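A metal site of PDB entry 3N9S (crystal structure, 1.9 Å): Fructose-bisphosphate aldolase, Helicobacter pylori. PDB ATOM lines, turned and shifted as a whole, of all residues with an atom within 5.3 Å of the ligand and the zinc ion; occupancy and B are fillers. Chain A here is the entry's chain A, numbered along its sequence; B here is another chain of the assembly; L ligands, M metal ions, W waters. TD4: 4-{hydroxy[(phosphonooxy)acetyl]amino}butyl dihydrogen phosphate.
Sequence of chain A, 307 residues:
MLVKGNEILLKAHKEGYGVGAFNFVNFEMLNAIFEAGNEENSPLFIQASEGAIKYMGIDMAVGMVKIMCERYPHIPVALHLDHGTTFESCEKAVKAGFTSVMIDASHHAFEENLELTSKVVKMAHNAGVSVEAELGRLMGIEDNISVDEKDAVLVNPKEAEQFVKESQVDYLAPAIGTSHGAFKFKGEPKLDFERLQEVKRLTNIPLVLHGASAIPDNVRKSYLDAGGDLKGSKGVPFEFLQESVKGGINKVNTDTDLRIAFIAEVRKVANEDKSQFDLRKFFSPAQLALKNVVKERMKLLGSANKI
Water W2 bridges an oxygen (O10) of the ligand (2.6 Å) and the backbone NH (N) of Gly 51 (3.0 Å). Water W5 lies within hydrogen-bond range of an oxygen (O18) of the ligand and the side-chain carboxylate (OD2) of Asp 255. Water W1 bridges an oxygen (O09) of the ligand (2.9 Å) and the side-chain hydroxyl of Ser 49 (3.4 Å). Water W6 lies within hydrogen-bond range of OD2 of Asp 255 (2.4 Å) and O07 of the ligand (3.0 Å).
Residues that only touch the zinc ion: Asn 253 (3.8 Å). Of the 24 residues printed, 4 come within 4 Å of the zinc ion. Along chain A the residues within 4 Å of the zinc ion span positions 83 to 253. The nearest printed residue that does not touch the zinc ion is Asp 82 (4.2 Å).
Asn 23 touches the ligand (OD1 to C03, 3.2 Å). Thr 254 touches the ligand (C to O19, 3.8 Å). Hydrophobic or aromatic side chains that line the ligand: His 83, His 180 and His 210. Of the 24 residues printed, 16 come within 4 Å of the ligand. Along chain A the residues within 4 Å of the ligand span positions 23 to 256.
The side-chain amino group (NZ) of Lys 184 lies within salt-bridge range of an oxygen (O17) of the ligand (2.6 Å). The side-chain hydroxyl (OG) of Ser 49 is in hydrogen-bond range of an oxygen (O09) of the ligand (2.6 Å). N of Ser 213 sits at hydrogen-bond distance from O17 of the ligand (2.8 Å). OG of Ser 213 is in hydrogen-bond range of O19 of the ligand, at 2.6 Å. An oxygen (O09) of the ligand is in salt-bridge range of the guanidinium group (NH1) of Arg 280 of chain B, 2.7 Å away. The side-chain carboxylate (OD2) of Asp 82 lies close to an oxygen (O01) of the ligand, 2.7 Å away. N of Thr 256 is in hydrogen-bond range of O19 of the ligand, 2.8 Å away. An oxygen (O18) of the ligand is in hydrogen-bond range of the side-chain hydroxyl (OG1) of Thr 256 (2.7 Å). An oxygen (O18) of the ligand lies within hydrogen-bond range of the backbone NH of Gly 181 (2.8 Å). An oxygen (O15) of the ligand lies close to the backbone NH (N) of Gly 211, at 3.1 Å. N of Asp 255 is in hydrogen-bond range of O19 of the ligand (2.9 Å). The backbone NH (N) of Ala 212 sits at hydrogen-bond distance from an oxygen (O17) of the ligand. The side-chain amide nitrogen of Asn 253 lies close to an oxygen (O01) of the ligand, at 3.1 Å.
The zinc ion is bound by an oxygen (O01) of the ligand (1.9 Å), a ring nitrogen (NE2) of His 180 (2.1 Å), a ring nitrogen (ND1) of His 210 (2.1 Å), a ring nitrogen (NE2) of His 83 (2.1 Å) and an oxygen (O13) of the ligand (2.6 Å). The zinc ion has five donor atoms within binding distance.
ND2 of Asn 253 lies close to NE2 of His 210 (3.4 Å). OG of Ser 49 is in hydrogen-bond range of N of Ala 52, at 3.0 Å. The backbone NH (N) of Asp 257 sits at hydrogen-bond distance from the side-chain hydroxyl (OG) of Ser 213, 3.0 Å away. NE of Arg 280 of chain B is in salt-bridge range of OD1 of Asp 278 of chain B. ND2 of Asn 23 sits at hydrogen-bond distance from OD2 of Asp 82. The side-chain amide nitrogen (NE2) of Gln 47 sits at hydrogen-bond distance from the side-chain carboxylate (OD2) of Asp 82 (3.5 Å). The backbone NH (N) of Asn 253 is in hydrogen-bond range of the backbone carbonyl oxygen (O) of Leu 209, at 3.0 Å. NE2 of Gln 47 lies within hydrogen-bond range of OD1 of Asn 23, 3.0 Å away.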
ATOM      1  N   ASN A  23      26.041 -15.775  22.995  1.00  0.00           N
ATOM      2  CA  ASN A  23      25.928 -16.751  24.076  1.00  0.00           C
ATOM      3  C   ASN A  23      25.071 -17.920  23.633  1.00  0.00           C
ATOM      4  O   ASN A  23      24.161 -17.775  22.794  1.00  0.00           O
ATOM      5  CB  ASN A  23      25.350 -16.108  25.341  1.00  0.00           C
ATOM      6  CG  ASN A  23      26.334 -15.186  26.038  1.00  0.00           C
ATOM      7  OD1 ASN A  23      26.623 -14.101  25.550  1.00  0.00           O
ATOM      8  ND2 ASN A  23      26.844 -15.610  27.182  1.00  0.00           N
ATOM      9  N   GLN A  47      30.234 -17.879  23.207  1.00  0.00           N
ATOM     10  CA  GLN A  47      30.460 -17.803  24.651  1.00  0.00           C
ATOM     11  C   GLN A  47      29.448 -18.537  25.519  1.00  0.00           C
ATOM     12  O   GLN A  47      28.279 -18.692  25.159  1.00  0.00           O
ATOM     13  CB  GLN A  47      30.597 -16.373  25.150  1.00  0.00           C
ATOM     14  CG  GLN A  47      30.016 -15.247  24.328  1.00  0.00           C
ATOM     15  CD  GLN A  47      30.414 -13.895  24.887  1.00  0.00           C
ATOM     16  OE1 GLN A  47      31.583 -13.494  24.820  1.00  0.00           O
ATOM     17  NE2 GLN A  47      29.457 -13.181  25.465  1.00  0.00           N
ATOM     18  N   SER A  49      28.329 -18.544  29.702  1.00  0.00           N
ATOM     19  CA  SER A  49      28.471 -18.060  31.069  1.00  0.00           C
ATOM     20  C   SER A  49      28.674 -19.231  32.030  1.00  0.00           C
ATOM     21  O   SER A  49      28.515 -20.403  31.677  1.00  0.00           O
ATOM     22  CB  SER A  49      27.190 -17.325  31.448  1.00  0.00           C
ATOM     23  OG  SER A  49      26.115 -18.260  31.468  1.00  0.00           O
ATOM     24  N   GLY A  51      26.696 -19.995  34.468  1.00  0.00           N
ATOM     25  CA  GLY A  51      25.380 -20.610  34.580  1.00  0.00           C
ATOM     26  C   GLY A  51      25.035 -21.495  33.394  1.00  0.00           C
ATOM     27  O   GLY A  51      24.305 -22.480  33.551  1.00  0.00           O
ATOM     28  N   ALA A  52      25.519 -21.154  32.214  1.00  0.00           N
ATOM     29  CA  ALA A  52      25.285 -21.977  31.030  1.00  0.00           C
ATOM     30  C   ALA A  52      26.153 -23.233  31.102  1.00  0.00           C
ATOM     31  O   ALA A  52      25.741 -24.309  30.679  1.00  0.00           O
ATOM     32  CB  ALA A  52      25.597 -21.205  29.767  1.00  0.00           C
ATOM     33  N   ASP A  82      32.285 -16.510  29.481  1.00  0.00           N
ATOM     34  CA  ASP A  82      31.698 -15.204  29.734  1.00  0.00           C
ATOM     35  C   ASP A  82      31.544 -14.996  31.233  1.00  0.00           C
ATOM     36  O   ASP A  82      31.097 -15.884  31.957  1.00  0.00           O
ATOM     37  CB  ASP A  82      30.339 -15.097  29.030  1.00  0.00           C
ATOM     38  CG  ASP A  82      29.801 -13.677  28.988  1.00  0.00           C
ATOM     39  OD1 ASP A  82      30.582 -12.713  29.143  1.00  0.00           O
ATOM     40  OD2 ASP A  82      28.582 -13.526  28.786  1.00  0.00           O
ATOM     41  N   HIS A  83      31.928 -13.810  31.695  1.00  0.00           N
ATOM     42  CA  HIS A  83      31.824 -13.462  33.110  1.00  0.00           C
ATOM     43  C   HIS A  83      32.310 -14.552  34.074  1.00  0.00           C
ATOM     44  O   HIS A  83      31.583 -14.968  34.968  1.00  0.00           O
ATOM     45  CB  HIS A  83      30.386 -13.068  33.447  1.00  0.00           C
ATOM     46  CG  HIS A  83      29.970 -11.782  32.803  1.00  0.00           C
ATOM     47  ND1 HIS A  83      30.437 -10.557  33.231  1.00  0.00           N
ATOM     48  CD2 HIS A  83      29.174 -11.524  31.743  1.00  0.00           C
ATOM     49  CE1 HIS A  83      29.935  -9.611  32.473  1.00  0.00           C
ATOM     50  NE2 HIS A  83      29.162 -10.164  31.568  1.00  0.00           N
ATOM     51  N   LEU A 138      28.374  -2.048  34.883  1.00  0.00           N
ATOM     52  CA  LEU A 138      27.495  -2.212  33.719  1.00  0.00           C
ATOM     53  C   LEU A 138      26.068  -1.802  34.030  1.00  0.00           C
ATOM     54  O   LEU A 138      25.160  -2.629  33.967  1.00  0.00           O
ATOM     55  CB  LEU A 138      27.487  -3.665  33.269  1.00  0.00           C
ATOM     56  CG  LEU A 138      28.505  -4.066  32.224  1.00  0.00           C
ATOM     57  CD1 LEU A 138      28.358  -5.559  31.950  1.00  0.00           C
ATOM     58  CD2 LEU A 138      28.326  -3.246  30.952  1.00  0.00           C
ATOM     59  N   SER A 179      24.176  -2.026  29.755  1.00  0.00           N
ATOM     60  CA  SER A 179      23.932  -2.972  30.832  1.00  0.00           C
ATOM     61  C   SER A 179      23.282  -4.202  30.228  1.00  0.00           C
ATOM     62  O   SER A 179      22.804  -4.159  29.085  1.00  0.00           O
ATOM     63  CB  SER A 179      23.013  -2.349  31.887  1.00  0.00           C
ATOM     64  OG  SER A 179      21.765  -2.019  31.316  1.00  0.00           O
ATOM     65  N   HIS A 180      23.270  -5.300  30.970  1.00  0.00           N
ATOM     66  CA  HIS A 180      22.677  -6.536  30.488  1.00  0.00           C
ATOM     67  C   HIS A 180      21.160  -6.471  30.440  1.00  0.00           C
ATOM     68  O   HIS A 180      20.533  -5.814  31.281  1.00  0.00           O
ATOM     69  CB  HIS A 180      23.081  -7.695  31.379  1.00  0.00           C
ATOM     70  CG  HIS A 180      24.539  -8.020  31.296  1.00  0.00           C
ATOM     71  ND1 HIS A 180      25.248  -8.513  32.363  1.00  0.00           N
ATOM     72  CD2 HIS A 180      25.411  -7.917  30.277  1.00  0.00           C
ATOM     73  CE1 HIS A 180      26.498  -8.711  32.001  1.00  0.00           C
ATOM     74  NE2 HIS A 180      26.628  -8.350  30.738  1.00  0.00           N
ATOM     75  N   GLY A 181      20.574  -7.142  29.468  1.00  0.00           N
ATOM     76  CA  GLY A 181      19.148  -7.388  29.464  1.00  0.00           C
ATOM     77  C   GLY A 181      18.349  -6.459  28.571  1.00  0.00           C
ATOM     78  O   GLY A 181      18.893  -5.596  27.878  1.00  0.00           O
ATOM     79  N   LYS A 184      17.552  -1.460  28.969  1.00  0.00           N
ATOM     80  CA  LYS A 184      18.809  -0.716  29.044  1.00  0.00           C
ATOM     81  C   LYS A 184      18.637   0.766  29.334  1.00  0.00           C
ATOM     82  O   LYS A 184      19.466   1.364  30.004  1.00  0.00           O
ATOM     83  CB  LYS A 184      19.614  -0.872  27.746  1.00  0.00           C
ATOM     84  CG  LYS A 184      20.002  -2.324  27.456  1.00  0.00           C
ATOM     85  CD  LYS A 184      20.988  -2.449  26.290  1.00  0.00           C
ATOM     86  CE  LYS A 184      20.977  -3.880  25.738  1.00  0.00           C
ATOM     87  NZ  LYS A 184      21.240  -4.890  26.825  1.00  0.00           N
ATOM     88  N   LEU A 209      32.319  -4.619  24.219  1.00  0.00           N
ATOM     89  CA  LEU A 209      31.087  -3.981  24.680  1.00  0.00           C
ATOM     90  C   LEU A 209      30.112  -5.039  25.197  1.00  0.00           C
ATOM     91  O   LEU A 209      29.651  -5.874  24.417  1.00  0.00           O
ATOM     92  CB  LEU A 209      30.433  -3.213  23.528  1.00  0.00           C
ATOM     93  CG  LEU A 209      29.170  -2.427  23.875  1.00  0.00           C
ATOM     94  CD1 LEU A 209      29.518  -1.216  24.705  1.00  0.00           C
ATOM     95  CD2 LEU A 209      28.441  -2.014  22.598  1.00  0.00           C
ATOM     96  N   HIS A 210      29.787  -4.992  26.475  1.00  0.00           N
ATOM     97  CA  HIS A 210      28.755  -5.874  27.047  1.00  0.00           C
ATOM     98  C   HIS A 210      27.428  -5.172  26.959  1.00  0.00           C
ATOM     99  O   HIS A 210      27.395  -3.954  26.790  1.00  0.00           O
ATOM    100  CB  HIS A 210      29.072  -6.177  28.515  1.00  0.00           C
ATOM    101  CG  HIS A 210      30.213  -7.123  28.684  1.00  0.00           C
ATOM    102  ND1 HIS A 210      30.071  -8.363  29.282  1.00  0.00           N
ATOM    103  CD2 HIS A 210      31.509  -7.031  28.317  1.00  0.00           C
ATOM    104  CE1 HIS A 210      31.237  -8.987  29.282  1.00  0.00           C
ATOM    105  NE2 HIS A 210      32.125  -8.199  28.703  1.00  0.00           N
ATOM    106  N   GLY A 211      26.342  -5.924  27.047  1.00  0.00           N
ATOM    107  CA  GLY A 211      25.004  -5.350  27.060  1.00  0.00           C
ATOM    108  C   GLY A 211      24.668  -4.712  25.726  1.00  0.00           C
ATOM    109  O   GLY A 211      23.991  -3.687  25.676  1.00  0.00           O
ATOM    110  N   ALA A 212      25.110  -5.331  24.638  1.00  0.00           N
ATOM    111  CA  ALA A 212      25.007  -4.732  23.301  1.00  0.00           C
ATOM    112  C   ALA A 212      23.822  -5.208  22.451  1.00  0.00           C
ATOM    113  O   ALA A 212      23.799  -4.975  21.241  1.00  0.00           O
ATOM    114  CB  ALA A 212      26.319  -4.957  22.547  1.00  0.00           C
ATOM    115  N   SER A 213      22.857  -5.895  23.057  1.00  0.00           N
ATOM    116  CA  SER A 213      21.643  -6.244  22.316  1.00  0.00           C
ATOM    117  C   SER A 213      20.908  -4.980  21.919  1.00  0.00           C
ATOM    118  O   SER A 213      20.976  -3.965  22.618  1.00  0.00           O
ATOM    119  CB  SER A 213      20.737  -7.145  23.142  1.00  0.00           C
ATOM    120  OG  SER A 213      21.195  -8.483  23.046  1.00  0.00           O
ATOM    121  N   ASN A 253      29.163  -8.330  22.740  1.00  0.00           N
ATOM    122  CA  ASN A 253      28.400  -9.375  23.430  1.00  0.00           C
ATOM    123  C   ASN A 253      26.915  -9.254  23.193  1.00  0.00           C
ATOM    124  O   ASN A 253      26.301  -8.242  23.571  1.00  0.00           O
ATOM    125  CB  ASN A 253      28.642  -9.316  24.943  1.00  0.00           C
ATOM    126  CG  ASN A 253      30.022  -9.740  25.339  1.00  0.00           C
ATOM    127  OD1 ASN A 253      30.940  -9.748  24.537  1.00  0.00           O
ATOM    128  ND2 ASN A 253      30.177 -10.084  26.614  1.00  0.00           N
ATOM    129  N   THR A 254      26.334 -10.306  22.622  1.00  0.00           N
ATOM    130  CA  THR A 254      24.938 -10.279  22.220  1.00  0.00           C
ATOM    131  C   THR A 254      24.303 -11.586  22.666  1.00  0.00           C
ATOM    132  O   THR A 254      24.714 -12.656  22.236  1.00  0.00           O
ATOM    133  CB  THR A 254      24.816 -10.193  20.704  1.00  0.00           C
ATOM    134  OG1 THR A 254      25.659  -9.140  20.234  1.00  0.00           O
ATOM    135  CG2 THR A 254      23.375  -9.931  20.304  1.00  0.00           C
ATOM    136  N   ASP A 255      23.272 -11.480  23.500  1.00  0.00           N
ATOM    137  CA  ASP A 255      22.642 -12.636  24.136  1.00  0.00           C
ATOM    138  C   ASP A 255      21.141 -12.419  24.145  1.00  0.00           C
ATOM    139  O   ASP A 255      20.374 -13.225  23.634  1.00  0.00           O
ATOM    140  CB  ASP A 255      23.182 -12.782  25.558  1.00  0.00           C
ATOM    141  CG  ASP A 255      22.412 -13.789  26.390  1.00  0.00           C
ATOM    142  OD1 ASP A 255      22.088 -14.891  25.889  1.00  0.00           O
ATOM    143  OD2 ASP A 255      22.125 -13.486  27.566  1.00  0.00           O
ATOM    144  N   THR A 256      20.719 -11.306  24.732  1.00  0.00           N
ATOM    145  CA  THR A 256      19.287 -11.028  24.886  1.00  0.00           C
ATOM    146  C   THR A 256      18.504 -11.086  23.559  1.00  0.00           C
ATOM    147  O   THR A 256      17.472 -11.741  23.485  1.00  0.00           O
ATOM    148  CB  THR A 256      19.081  -9.693  25.592  1.00  0.00           C
ATOM    149  OG1 THR A 256      19.508  -9.826  26.958  1.00  0.00           O
ATOM    150  CG2 THR A 256      17.631  -9.282  25.566  1.00  0.00           C
ATOM    151  N   ASP A 257      18.998 -10.425  22.517  1.00  0.00           N
ATOM    152  CA  ASP A 257      18.343 -10.455  21.192  1.00  0.00           C
ATOM    153  C   ASP A 257      18.114 -11.868  20.682  1.00  0.00           C
ATOM    154  O   ASP A 257      17.072 -12.163  20.078  1.00  0.00           O
ATOM    155  CB  ASP A 257      19.167  -9.731  20.142  1.00  0.00           C
ATOM    156  CG  ASP A 257      19.109  -8.241  20.279  1.00  0.00           C
ATOM    157  OD1 ASP A 257      18.230  -7.752  21.017  1.00  0.00           O
ATOM    158  OD2 ASP A 257      19.939  -7.567  19.629  1.00  0.00           O
ATOM    159  N   ASP B 278      14.337 -16.682  29.031  1.00  0.00           N
ATOM    160  CA  ASP B 278      15.520 -17.463  29.339  1.00  0.00           C
ATOM    161  C   ASP B 278      15.214 -18.914  28.973  1.00  0.00           C
ATOM    162  O   ASP B 278      14.337 -19.542  29.590  1.00  0.00           O
ATOM    163  CB  ASP B 278      15.848 -17.355  30.839  1.00  0.00           C
ATOM    164  CG  ASP B 278      17.093 -18.128  31.230  1.00  0.00           C
ATOM    165  OD1 ASP B 278      17.579 -18.977  30.442  1.00  0.00           O
ATOM    166  OD2 ASP B 278      17.609 -17.903  32.347  1.00  0.00           O
ATOM    167  N   ARG B 280      16.602 -21.596  29.605  1.00  0.00           N
ATOM    168  CA  ARG B 280      16.777 -22.566  30.688  1.00  0.00           C
ATOM    169  C   ARG B 280      15.540 -22.657  31.575  1.00  0.00           C
ATOM    170  O   ARG B 280      15.213 -23.725  32.100  1.00  0.00           O
ATOM    171  CB  ARG B 280      18.011 -22.217  31.512  1.00  0.00           C
ATOM    172  CG  ARG B 280      19.302 -22.408  30.745  1.00  0.00           C
ATOM    173  CD  ARG B 280      20.433 -21.613  31.388  1.00  0.00           C
ATOM    174  NE  ARG B 280      20.165 -20.180  31.325  1.00  0.00           N
ATOM    175  CZ  ARG B 280      21.007 -19.242  31.735  1.00  0.00           C
ATOM    176  NH1 ARG B 280      22.181 -19.589  32.240  1.00  0.00           N
ATOM    177  NH2 ARG B 280      20.675 -17.957  31.640  1.00  0.00           N
HETATM  178  O01 TD4 L   1      28.111 -10.872  28.804  1.00  0.00           O
HETATM  179  N02 TD4 L   1      26.998 -10.843  27.969  1.00  0.00           N
HETATM  180  C03 TD4 L   1      26.176 -12.030  27.919  1.00  0.00           C
HETATM  181  C04 TD4 L   1      25.273 -12.155  29.143  1.00  0.00           C
HETATM  182  C05 TD4 L   1      25.534 -13.349  30.037  1.00  0.00           C
HETATM  183  C06 TD4 L   1      24.438 -13.682  31.023  1.00  0.00           C
HETATM  184  O07 TD4 L   1      23.890 -14.955  30.891  1.00  0.00           O
HETATM  185  P08 TD4 L   1      23.581 -15.823  32.244  1.00  0.00           P
HETATM  186  O09 TD4 L   1      23.711 -17.406  31.873  1.00  0.00           O
HETATM  187  O10 TD4 L   1      24.670 -15.420  33.395  1.00  0.00           O
HETATM  188  O11 TD4 L   1      22.243 -15.498  32.722  1.00  0.00           O
HETATM  189  C12 TD4 L   1      26.404  -9.580  27.590  1.00  0.00           C
HETATM  190  O13 TD4 L   1      27.020  -8.570  27.724  1.00  0.00           O
HETATM  191  C14 TD4 L   1      25.094  -9.617  26.791  1.00  0.00           C
HETATM  192  O15 TD4 L   1      24.460  -8.386  26.634  1.00  0.00           O
HETATM  193  P16 TD4 L   1      22.856  -8.295  26.235  1.00  0.00           P
HETATM  194  O17 TD4 L   1      22.611  -6.762  25.712  1.00  0.00           O
HETATM  195  O18 TD4 L   1      21.915  -8.650  27.518  1.00  0.00           O
HETATM  196  O19 TD4 L   1      22.578  -9.199  25.122  1.00  0.00           O
HETATM  197 ZN    ZN M   1      28.271  -9.266  29.841  1.00  0.00          ZN
HETATM  198  O   HOH W   1      23.722 -17.881  29.053  1.00  0.00           O
HETATM  199  O   HOH W   2      25.947 -17.140  34.816  1.00  0.00           O
HETATM  200  O   HOH W   3      20.308 -13.640  32.252  1.00  0.00           O
HETATM  201  O   HOH W   4      20.881 -16.029  34.910  1.00  0.00           O
HETATM  202  O   HOH W   5      22.260 -11.043  28.835  1.00  0.00           O
HETATM  203  O   HOH W   6      21.436 -15.194  29.155  1.00  0.00           O
HETATM  204  O   HOH W   7      27.194 -14.284  33.045  1.00  0.00           O
HETATM  205  O   HOH W   8      24.238 -13.361  34.893  1.00  0.00           O
